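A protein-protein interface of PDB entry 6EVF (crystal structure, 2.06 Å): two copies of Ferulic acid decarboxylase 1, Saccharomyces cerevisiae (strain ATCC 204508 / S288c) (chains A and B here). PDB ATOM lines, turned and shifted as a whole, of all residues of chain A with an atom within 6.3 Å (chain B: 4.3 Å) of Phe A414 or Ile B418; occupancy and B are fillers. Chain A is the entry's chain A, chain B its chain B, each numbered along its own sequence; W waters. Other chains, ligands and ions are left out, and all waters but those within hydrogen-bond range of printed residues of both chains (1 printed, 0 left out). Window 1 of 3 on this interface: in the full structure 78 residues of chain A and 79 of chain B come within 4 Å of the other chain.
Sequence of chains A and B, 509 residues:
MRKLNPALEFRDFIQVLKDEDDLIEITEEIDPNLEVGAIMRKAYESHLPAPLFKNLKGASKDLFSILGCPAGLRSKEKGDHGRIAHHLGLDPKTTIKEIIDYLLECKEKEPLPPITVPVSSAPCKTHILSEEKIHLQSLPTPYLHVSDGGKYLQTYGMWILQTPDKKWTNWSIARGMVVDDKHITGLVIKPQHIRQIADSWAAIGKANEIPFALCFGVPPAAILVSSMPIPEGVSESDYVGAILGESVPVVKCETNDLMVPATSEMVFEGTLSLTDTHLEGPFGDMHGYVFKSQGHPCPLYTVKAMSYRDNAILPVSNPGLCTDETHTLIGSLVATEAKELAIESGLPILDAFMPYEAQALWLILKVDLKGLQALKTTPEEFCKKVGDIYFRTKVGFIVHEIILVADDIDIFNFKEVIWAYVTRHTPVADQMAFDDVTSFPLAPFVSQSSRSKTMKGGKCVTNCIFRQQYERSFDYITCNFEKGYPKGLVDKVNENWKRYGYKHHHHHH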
ATOM      1  N   CYS A 322      -2.561  -0.071  31.294  1.00  0.00           N
ATOM      2  CA  CYS A 322      -1.396   0.811  31.168  1.00  0.00           C
ATOM      3  C   CYS A 322      -1.173   1.486  32.560  1.00  0.00           C
ATOM      4  O   CYS A 322      -2.114   1.629  33.292  1.00  0.00           O
ATOM      5  CB  CYS A 322      -1.616   1.803  30.031  1.00  0.00           C
ATOM      6  SG  CYS A 322      -3.063   2.865  30.242  1.00  0.00           S
ATOM      7  N   PRO A 355       1.355   4.804  21.939  1.00  0.00           N
ATOM      8  CA  PRO A 355       0.718   5.314  23.136  1.00  0.00           C
ATOM      9  C   PRO A 355       0.382   4.243  24.182  1.00  0.00           C
ATOM     10  O   PRO A 355      -0.238   3.200  23.867  1.00  0.00           O
ATOM     11  CB  PRO A 355      -0.540   5.981  22.606  1.00  0.00           C
ATOM     12  CG  PRO A 355      -0.270   6.259  21.163  1.00  0.00           C
ATOM     13  CD  PRO A 355       0.625   5.158  20.726  1.00  0.00           C
ATOM     14  N   TYR A 356       0.734   4.543  25.421  1.00  0.00           N
ATOM     15  CA  TYR A 356       0.477   3.633  26.514  1.00  0.00           C
ATOM     16  C   TYR A 356      -1.001   3.301  26.693  1.00  0.00           C
ATOM     17  O   TYR A 356      -1.379   2.134  26.860  1.00  0.00           O
ATOM     18  CB  TYR A 356       1.120   4.088  27.823  1.00  0.00           C
ATOM     19  CG  TYR A 356       2.571   4.513  27.690  1.00  0.00           C
ATOM     20  CD1 TYR A 356       3.469   3.747  26.952  1.00  0.00           C
ATOM     21  CD2 TYR A 356       3.020   5.739  28.242  1.00  0.00           C
ATOM     22  CE1 TYR A 356       4.772   4.138  26.804  1.00  0.00           C
ATOM     23  CE2 TYR A 356       4.323   6.158  28.082  1.00  0.00           C
ATOM     24  CZ  TYR A 356       5.181   5.335  27.361  1.00  0.00           C
ATOM     25  OH  TYR A 356       6.460   5.683  27.140  1.00  0.00           O
ATOM     26  N   GLU A 357      -1.824   4.298  26.507  1.00  0.00           N
ATOM     27  CA  GLU A 357      -3.284   4.214  26.642  1.00  0.00           C
ATOM     28  C   GLU A 357      -3.931   3.256  25.689  1.00  0.00           C
ATOM     29  O   GLU A 357      -4.999   2.729  25.986  1.00  0.00           O
ATOM     30  CB  GLU A 357      -3.914   5.619  26.533  1.00  0.00           C
ATOM     31  CG  GLU A 357      -3.465   6.523  27.680  1.00  0.00           C
ATOM     32  CD  GLU A 357      -2.190   7.327  27.459  1.00  0.00           C
ATOM     33  OE1 GLU A 357      -1.389   7.082  26.480  1.00  0.00           O
ATOM     34  OE2 GLU A 357      -2.002   8.243  28.311  1.00  0.00           O
ATOM     35  N   ALA A 358      -3.250   2.965  24.579  1.00  0.00           N
ATOM     36  CA  ALA A 358      -3.714   2.040  23.613  1.00  0.00           C
ATOM     37  C   ALA A 358      -3.053   0.641  23.754  1.00  0.00           C
ATOM     38  O   ALA A 358      -3.166  -0.185  22.861  1.00  0.00           O
ATOM     39  CB  ALA A 358      -3.547   2.618  22.211  1.00  0.00           C
ATOM     40  N   GLN A 359      -2.477   0.349  24.914  1.00  0.00           N
ATOM     41  CA  GLN A 359      -2.012  -0.994  25.276  1.00  0.00           C
ATOM     42  C   GLN A 359      -1.071  -1.569  24.252  1.00  0.00           C
ATOM     43  O   GLN A 359      -1.129  -2.751  23.968  1.00  0.00           O
ATOM     44  CB  GLN A 359      -3.201  -1.919  25.495  1.00  0.00           C
ATOM     45  CG  GLN A 359      -4.236  -1.450  26.505  1.00  0.00           C
ATOM     46  CD  GLN A 359      -3.728  -1.494  27.946  1.00  0.00           C
ATOM     47  OE1 GLN A 359      -2.892  -2.366  28.365  1.00  0.00           O
ATOM     48  NE2 GLN A 359      -4.196  -0.562  28.700  1.00  0.00           N
ATOM     49  N   TRP A 362      -1.409   0.487  19.090  1.00  0.00           N
ATOM     50  CA  TRP A 362      -1.467   1.609  18.151  1.00  0.00           C
ATOM     51  C   TRP A 362      -0.079   2.068  17.934  1.00  0.00           C
ATOM     52  O   TRP A 362       0.649   2.279  18.887  1.00  0.00           O
ATOM     53  CB  TRP A 362      -2.235   2.806  18.736  1.00  0.00           C
ATOM     54  CG  TRP A 362      -3.721   2.685  18.684  1.00  0.00           C
ATOM     55  CD1 TRP A 362      -4.441   1.571  18.391  1.00  0.00           C
ATOM     56  CD2 TRP A 362      -4.654   3.703  18.939  1.00  0.00           C
ATOM     57  NE1 TRP A 362      -5.774   1.854  18.399  1.00  0.00           N
ATOM     58  CE2 TRP A 362      -5.939   3.147  18.769  1.00  0.00           C
ATOM     59  CE3 TRP A 362      -4.546   5.030  19.319  1.00  0.00           C
ATOM     60  CZ2 TRP A 362      -7.130   3.909  18.901  1.00  0.00           C
ATOM     61  CZ3 TRP A 362      -5.700   5.771  19.493  1.00  0.00           C
ATOM     62  CH2 TRP A 362      -6.995   5.196  19.272  1.00  0.00           C
ATOM     63  N   ASP A 410       1.942  16.441  18.922  1.00  0.00           N
ATOM     64  CA  ASP A 410       2.909  15.838  19.835  1.00  0.00           C
ATOM     65  C   ASP A 410       2.439  14.397  20.127  1.00  0.00           C
ATOM     66  O   ASP A 410       1.619  14.158  21.025  1.00  0.00           O
ATOM     67  CB  ASP A 410       3.111  16.648  21.126  1.00  0.00           C
ATOM     68  CG  ASP A 410       4.161  15.995  22.049  1.00  0.00           C
ATOM     69  OD1 ASP A 410       4.813  14.996  21.664  1.00  0.00           O
ATOM     70  OD2 ASP A 410       4.323  16.480  23.154  1.00  0.00           O
ATOM     71  N   ILE A 411       2.958  13.451  19.335  1.00  0.00           N
ATOM     72  CA  ILE A 411       2.511  12.049  19.410  1.00  0.00           C
ATOM     73  C   ILE A 411       2.825  11.379  20.756  1.00  0.00           C
ATOM     74  O   ILE A 411       2.268  10.349  21.045  1.00  0.00           O
ATOM     75  CB  ILE A 411       3.061  11.179  18.254  1.00  0.00           C
ATOM     76  CG1 ILE A 411       4.592  10.999  18.355  1.00  0.00           C
ATOM     77  CG2 ILE A 411       2.640  11.728  16.920  1.00  0.00           C
ATOM     78  CD1 ILE A 411       5.179  10.079  17.324  1.00  0.00           C
ATOM     79  N   PHE A 412       3.696  12.011  21.571  1.00  0.00           N
ATOM     80  CA  PHE A 412       4.110  11.477  22.857  1.00  0.00           C
ATOM     81  C   PHE A 412       3.187  11.875  23.971  1.00  0.00           C
ATOM     82  O   PHE A 412       3.342  11.414  25.069  1.00  0.00           O
ATOM     83  CB  PHE A 412       5.569  11.895  23.148  1.00  0.00           C
ATOM     84  CG  PHE A 412       6.522  11.445  22.096  1.00  0.00           C
ATOM     85  CD1 PHE A 412       6.928  10.127  22.048  1.00  0.00           C
ATOM     86  CD2 PHE A 412       6.970  12.349  21.118  1.00  0.00           C
ATOM     87  CE1 PHE A 412       7.806   9.688  21.075  1.00  0.00           C
ATOM     88  CE2 PHE A 412       7.847  11.942  20.154  1.00  0.00           C
ATOM     89  CZ  PHE A 412       8.254  10.586  20.113  1.00  0.00           C
ATOM     90  N   ASN A 413       2.213  12.717  23.661  1.00  0.00           N
ATOM     91  CA  ASN A 413       1.199  13.168  24.563  1.00  0.00           C
ATOM     92  C   ASN A 413      -0.165  12.679  24.000  1.00  0.00           C
ATOM     93  O   ASN A 413      -0.637  13.137  22.951  1.00  0.00           O
ATOM     94  CB  ASN A 413       1.250  14.702  24.552  1.00  0.00           C
ATOM     95  CG  ASN A 413       0.206  15.341  25.453  1.00  0.00           C
ATOM     96  OD1 ASN A 413      -0.662  14.693  26.025  1.00  0.00           O
ATOM     97  ND2 ASN A 413       0.281  16.630  25.544  1.00  0.00           N
ATOM     98  N   PHE A 414      -0.843  11.827  24.753  1.00  0.00           N
ATOM     99  CA  PHE A 414      -2.074  11.224  24.316  1.00  0.00           C
ATOM    100  C   PHE A 414      -3.254  12.209  24.232  1.00  0.00           C
ATOM    101  O   PHE A 414      -4.163  11.983  23.426  1.00  0.00           O
ATOM    102  CB  PHE A 414      -2.415  10.039  25.216  1.00  0.00           C
ATOM    103  CG  PHE A 414      -3.469   9.135  24.634  1.00  0.00           C
ATOM    104  CD1 PHE A 414      -3.244   8.471  23.409  1.00  0.00           C
ATOM    105  CD2 PHE A 414      -4.712   9.001  25.246  1.00  0.00           C
ATOM    106  CE1 PHE A 414      -4.217   7.656  22.859  1.00  0.00           C
ATOM    107  CE2 PHE A 414      -5.680   8.184  24.688  1.00  0.00           C
ATOM    108  CZ  PHE A 414      -5.430   7.528  23.489  1.00  0.00           C
ATOM    109  N   LYS A 415      -3.227  13.319  24.969  1.00  0.00           N
ATOM    110  CA  LYS A 415      -4.249  14.367  24.774  1.00  0.00           C
ATOM    111  C   LYS A 415      -4.255  14.884  23.324  1.00  0.00           C
ATOM    112  O   LYS A 415      -5.293  15.154  22.787  1.00  0.00           O
ATOM    113  CB  LYS A 415      -4.060  15.533  25.728  1.00  0.00           C
ATOM    114  CG  LYS A 415      -4.156  15.170  27.211  1.00  0.00           C
ATOM    115  CD  LYS A 415      -4.142  16.477  28.027  1.00  0.00           C
ATOM    116  CE  LYS A 415      -4.338  16.269  29.538  1.00  0.00           C
ATOM    117  NZ  LYS A 415      -4.099  17.532  30.312  1.00  0.00           N
ATOM    118  N   GLU A 416      -3.082  15.021  22.703  1.00  0.00           N
ATOM    119  CA  GLU A 416      -2.998  15.481  21.314  1.00  0.00           C
ATOM    120  C   GLU A 416      -3.350  14.330  20.384  1.00  0.00           C
ATOM    121  O   GLU A 416      -4.001  14.549  19.395  1.00  0.00           O
ATOM    122  CB  GLU A 416      -1.608  16.047  20.970  1.00  0.00           C
ATOM    123  CG  GLU A 416      -1.179  17.153  21.905  1.00  0.00           C
ATOM    124  CD  GLU A 416      -0.259  18.229  21.281  1.00  0.00           C
ATOM    125  OE1 GLU A 416       0.041  18.278  20.039  1.00  0.00           O
ATOM    126  OE2 GLU A 416       0.226  19.013  22.103  1.00  0.00           O
ATOM    127  N   VAL A 417      -2.948  13.115  20.718  1.00  0.00           N
ATOM    128  CA  VAL A 417      -3.208  11.982  19.833  1.00  0.00           C
ATOM    129  C   VAL A 417      -4.706  11.698  19.722  1.00  0.00           C
ATOM    130  O   VAL A 417      -5.235  11.499  18.631  1.00  0.00           O
ATOM    131  CB  VAL A 417      -2.475  10.711  20.301  1.00  0.00           C
ATOM    132  CG1 VAL A 417      -2.829   9.524  19.438  1.00  0.00           C
ATOM    133  CG2 VAL A 417      -0.972  10.930  20.217  1.00  0.00           C
ATOM    134  N   ILE A 418      -5.377  11.599  20.855  1.00  0.00           N
ATOM    135  CA  ILE A 418      -6.762  11.222  20.832  1.00  0.00           C
ATOM    136  C   ILE A 418      -7.537  12.372  20.161  1.00  0.00           C
ATOM    137  O   ILE A 418      -8.438  12.102  19.448  1.00  0.00           O
ATOM    138  CB  ILE A 418      -7.306  10.875  22.217  1.00  0.00           C
ATOM    139  CG1 ILE A 418      -8.687  10.174  22.133  1.00  0.00           C
ATOM    140  CG2 ILE A 418      -7.430  12.122  23.097  1.00  0.00           C
ATOM    141  CD1 ILE A 418      -8.653   8.883  21.336  1.00  0.00           C
ATOM    142  N   TRP A 419      -7.116  13.635  20.333  1.00  0.00           N
ATOM    143  CA  TRP A 419      -7.734  14.774  19.635  1.00  0.00           C
ATOM    144  C   TRP A 419      -7.671  14.605  18.140  1.00  0.00           C
ATOM    145  O   TRP A 419      -8.677  14.742  17.430  1.00  0.00           O
ATOM    146  CB  TRP A 419      -7.051  16.117  20.046  1.00  0.00           C
ATOM    147  CG  TRP A 419      -7.492  17.263  19.347  1.00  0.00           C
ATOM    148  CD1 TRP A 419      -8.758  17.701  19.228  1.00  0.00           C
ATOM    149  CD2 TRP A 419      -6.679  18.134  18.574  1.00  0.00           C
ATOM    150  NE1 TRP A 419      -8.797  18.832  18.435  1.00  0.00           N
ATOM    151  CE2 TRP A 419      -7.519  19.113  18.023  1.00  0.00           C
ATOM    152  CE3 TRP A 419      -5.299  18.210  18.339  1.00  0.00           C
ATOM    153  CZ2 TRP A 419      -7.036  20.172  17.273  1.00  0.00           C
ATOM    154  CZ3 TRP A 419      -4.815  19.229  17.566  1.00  0.00           C
ATOM    155  CH2 TRP A 419      -5.687  20.207  17.022  1.00  0.00           C
ATOM    156  N   PHE B 414     -12.799   7.681  31.157  1.00  0.00           N
ATOM    157  CA  PHE B 414     -12.210   7.473  29.831  1.00  0.00           C
ATOM    158  C   PHE B 414     -11.038   6.453  29.793  1.00  0.00           C
ATOM    159  O   PHE B 414     -10.801   5.867  28.752  1.00  0.00           O
ATOM    160  CB  PHE B 414     -11.781   8.772  29.209  1.00  0.00           C
ATOM    161  CG  PHE B 414     -11.444   8.651  27.742  1.00  0.00           C
ATOM    162  CD1 PHE B 414     -12.448   8.345  26.795  1.00  0.00           C
ATOM    163  CD2 PHE B 414     -10.145   8.875  27.304  1.00  0.00           C
ATOM    164  CE1 PHE B 414     -12.155   8.205  25.430  1.00  0.00           C
ATOM    165  CE2 PHE B 414      -9.849   8.797  25.949  1.00  0.00           C
ATOM    166  CZ  PHE B 414     -10.846   8.449  25.007  1.00  0.00           C
ATOM    167  N   LYS B 415     -10.358   6.229  30.912  1.00  0.00           N
ATOM    168  CA  LYS B 415      -9.366   5.144  31.029  1.00  0.00           C
ATOM    169  C   LYS B 415      -9.948   3.803  30.750  1.00  0.00           C
ATOM    170  O   LYS B 415      -9.335   3.032  30.032  1.00  0.00           O
ATOM    171  CB  LYS B 415      -8.740   5.057  32.410  1.00  0.00           C
ATOM    172  CG  LYS B 415      -7.878   6.230  32.773  1.00  0.00           C
ATOM    173  CD  LYS B 415      -7.244   6.026  34.146  1.00  0.00           C
ATOM    174  CE  LYS B 415      -6.235   7.138  34.393  1.00  0.00           C
ATOM    175  NZ  LYS B 415      -6.141   7.370  35.847  1.00  0.00           N
ATOM    176  N   GLU B 416     -11.150   3.539  31.251  1.00  0.00           N
ATOM    177  CA  GLU B 416     -11.812   2.281  30.906  1.00  0.00           C
ATOM    178  C   GLU B 416     -12.363   2.255  29.492  1.00  0.00           C
ATOM    179  O   GLU B 416     -12.369   1.219  28.855  1.00  0.00           O
ATOM    180  CB  GLU B 416     -12.914   1.989  31.906  1.00  0.00           C
ATOM    181  CG  GLU B 416     -12.357   1.778  33.315  1.00  0.00           C
ATOM    182  CD  GLU B 416     -13.355   1.157  34.281  1.00  0.00           C
ATOM    183  OE1 GLU B 416     -14.217   0.285  33.905  1.00  0.00           O
ATOM    184  OE2 GLU B 416     -13.275   1.526  35.470  1.00  0.00           O
ATOM    185  N   VAL B 417     -12.858   3.367  29.007  1.00  0.00           N
ATOM    186  CA  VAL B 417     -13.421   3.437  27.632  1.00  0.00           C
ATOM    187  C   VAL B 417     -12.313   3.175  26.577  1.00  0.00           C
ATOM    188  O   VAL B 417     -12.514   2.350  25.662  1.00  0.00           O
ATOM    189  CB  VAL B 417     -14.120   4.795  27.334  1.00  0.00           C
ATOM    190  CG1 VAL B 417     -14.509   4.911  25.874  1.00  0.00           C
ATOM    191  CG2 VAL B 417     -15.351   4.999  28.230  1.00  0.00           C
ATOM    192  N   ILE B 418     -11.177   3.857  26.697  1.00  0.00           N
ATOM    193  CA  ILE B 418     -10.104   3.703  25.703  1.00  0.00           C
ATOM    194  C   ILE B 418      -9.520   2.292  25.769  1.00  0.00           C
ATOM    195  O   ILE B 418      -9.195   1.714  24.745  1.00  0.00           O
ATOM    196  CB  ILE B 418      -8.970   4.796  25.828  1.00  0.00           C
ATOM    197  CG1 ILE B 418      -8.112   4.828  24.587  1.00  0.00           C
ATOM    198  CG2 ILE B 418      -8.043   4.608  27.010  1.00  0.00           C
ATOM    199  CD1 ILE B 418      -8.901   5.096  23.352  1.00  0.00           C
ATOM    200  N   TRP B 419      -9.419   1.728  26.972  1.00  0.00           N
ATOM    201  CA  TRP B 419      -8.986   0.339  27.122  1.00  0.00           C
ATOM    202  C   TRP B 419      -9.907  -0.617  26.423  1.00  0.00           C
ATOM    203  O   TRP B 419      -9.471  -1.443  25.638  1.00  0.00           O
ATOM    204  CB  TRP B 419      -8.872  -0.049  28.594  1.00  0.00           C
ATOM    205  CG  TRP B 419      -8.602  -1.508  28.830  1.00  0.00           C
ATOM    206  CD1 TRP B 419      -7.541  -2.219  28.421  1.00  0.00           C
ATOM    207  CD2 TRP B 419      -9.424  -2.403  29.568  1.00  0.00           C
ATOM    208  NE1 TRP B 419      -7.671  -3.519  28.834  1.00  0.00           N
ATOM    209  CE2 TRP B 419      -8.795  -3.625  29.589  1.00  0.00           C
ATOM    210  CE3 TRP B 419     -10.622  -2.261  30.255  1.00  0.00           C
ATOM    211  CZ2 TRP B 419      -9.342  -4.721  30.223  1.00  0.00           C
ATOM    212  CZ3 TRP B 419     -11.143  -3.348  30.847  1.00  0.00           C
ATOM    213  CH2 TRP B 419     -10.519  -4.546  30.844  1.00  0.00           C
ATOM    214  N   ALA B 420     -11.189  -0.486  26.676  1.00  0.00           N
ATOM    215  CA  ALA B 420     -12.195  -1.299  25.985  1.00  0.00           C
ATOM    216  C   ALA B 420     -12.214  -1.067  24.480  1.00  0.00           C
ATOM    217  O   ALA B 420     -12.362  -1.995  23.738  1.00  0.00           O
ATOM    218  CB  ALA B 420     -13.576  -1.032  26.565  1.00  0.00           C
ATOM    219  N   TYR B 421     -12.085   0.184  24.035  1.00  0.00           N
ATOM    220  CA  TYR B 421     -12.052   0.492  22.621  1.00  0.00           C
ATOM    221  C   TYR B 421     -10.936  -0.260  21.880  1.00  0.00           C
ATOM    222  O   TYR B 421     -11.204  -0.996  20.909  1.00  0.00           O
ATOM    223  CB  TYR B 421     -11.917   1.975  22.391  1.00  0.00           C
ATOM    224  CG  TYR B 421     -12.104   2.410  20.962  1.00  0.00           C
ATOM    225  CD1 TYR B 421     -13.383   2.516  20.434  1.00  0.00           C
ATOM    226  CD2 TYR B 421     -11.007   2.743  20.146  1.00  0.00           C
ATOM    227  CE1 TYR B 421     -13.571   2.930  19.122  1.00  0.00           C
ATOM    228  CE2 TYR B 421     -11.180   3.159  18.839  1.00  0.00           C
ATOM    229  CZ  TYR B 421     -12.461   3.232  18.322  1.00  0.00           C
ATOM    230  OH  TYR B 421     -12.742   3.655  17.045  1.00  0.00           O
ATOM    231  N   VAL B 422      -9.712  -0.121  22.365  1.00  0.00           N
ATOM    232  CA  VAL B 422      -8.604  -0.675  21.678  1.00  0.00           C
ATOM    233  C   VAL B 422      -8.480  -2.177  21.822  1.00  0.00           C
ATOM    234  O   VAL B 422      -7.985  -2.793  20.912  1.00  0.00           O
ATOM    235  CB  VAL B 422      -7.283   0.008  22.019  1.00  0.00           C
ATOM    236  CG1 VAL B 422      -7.395   1.529  21.800  1.00  0.00           C
ATOM    237  CG2 VAL B 422      -6.801  -0.370  23.423  1.00  0.00           C
HETATM  238  O   HOH W   1      -6.543   3.061  30.310  1.00  0.00           O
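The backbone NH (N) of Cys A322 sits close to the side-chain amide nitrogen (NE2) of Gln A359 (3.1 Å).
Among the printed residues, pairs that only touch across the chains: Glu A357 with Ile B418 (3.7 Å), Ala A358 with Val B422 (3.7 Å), Gln A359 with Trp B419 (3.7 Å), Trp A362 with Val B422 (3.7 Å), Phe A414 with Ile B418 (3.96 Å) and Ile A418 with Phe B414 (3.99 Å).
Of chain B, only Ile B418 (3.96 Å) comes within 4 Å of Phe A414. Ile B418 touches two residues of chain A. Printed residues of chain B within 4 Å of Glu A357: Ile B418. Printed residues of chain B within 4 Å of Ile A418: Phe B414 (3.99 Å). Printed residues of chain B within 4 Å of Ala A358: Val B422 (3.7 Å). Of the printed residues of chain A, Phe B414 touches Ile A418 (3.99 Å). Lys B415 touches none of the printed residues of chain A. Asn A413 touches none of the printed residues of chain B. The nearest residue of chain A that does not touch Ile B418 is Ile A418 (4.3 Å). The nearest printed residue of chain A that does not touch Val B422 is Gln A359 (4.2 Å).
Along chain A the printed residues that touch a printed residue of chain B span positions 357 to 418. Among the printed residues, 6 pairs touch across the chains. Among the printed residues, no Asp or Glu carboxylate lies within 4 Å of a Lys or Arg side-chain nitrogen of the other chain.
Phe A414 touches Ile B418, and with the chains exchanged Ile A418 touches Phe B414. 6 positions are printed for both chains. Of the 6 pairs that touch across the chains among the printed residues, 2 have their exchanged pair printed and touching as well.
Water W1 bridges O of Lys B415 (2.8 Å) and SG of Cys A322 (3.5 Å).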
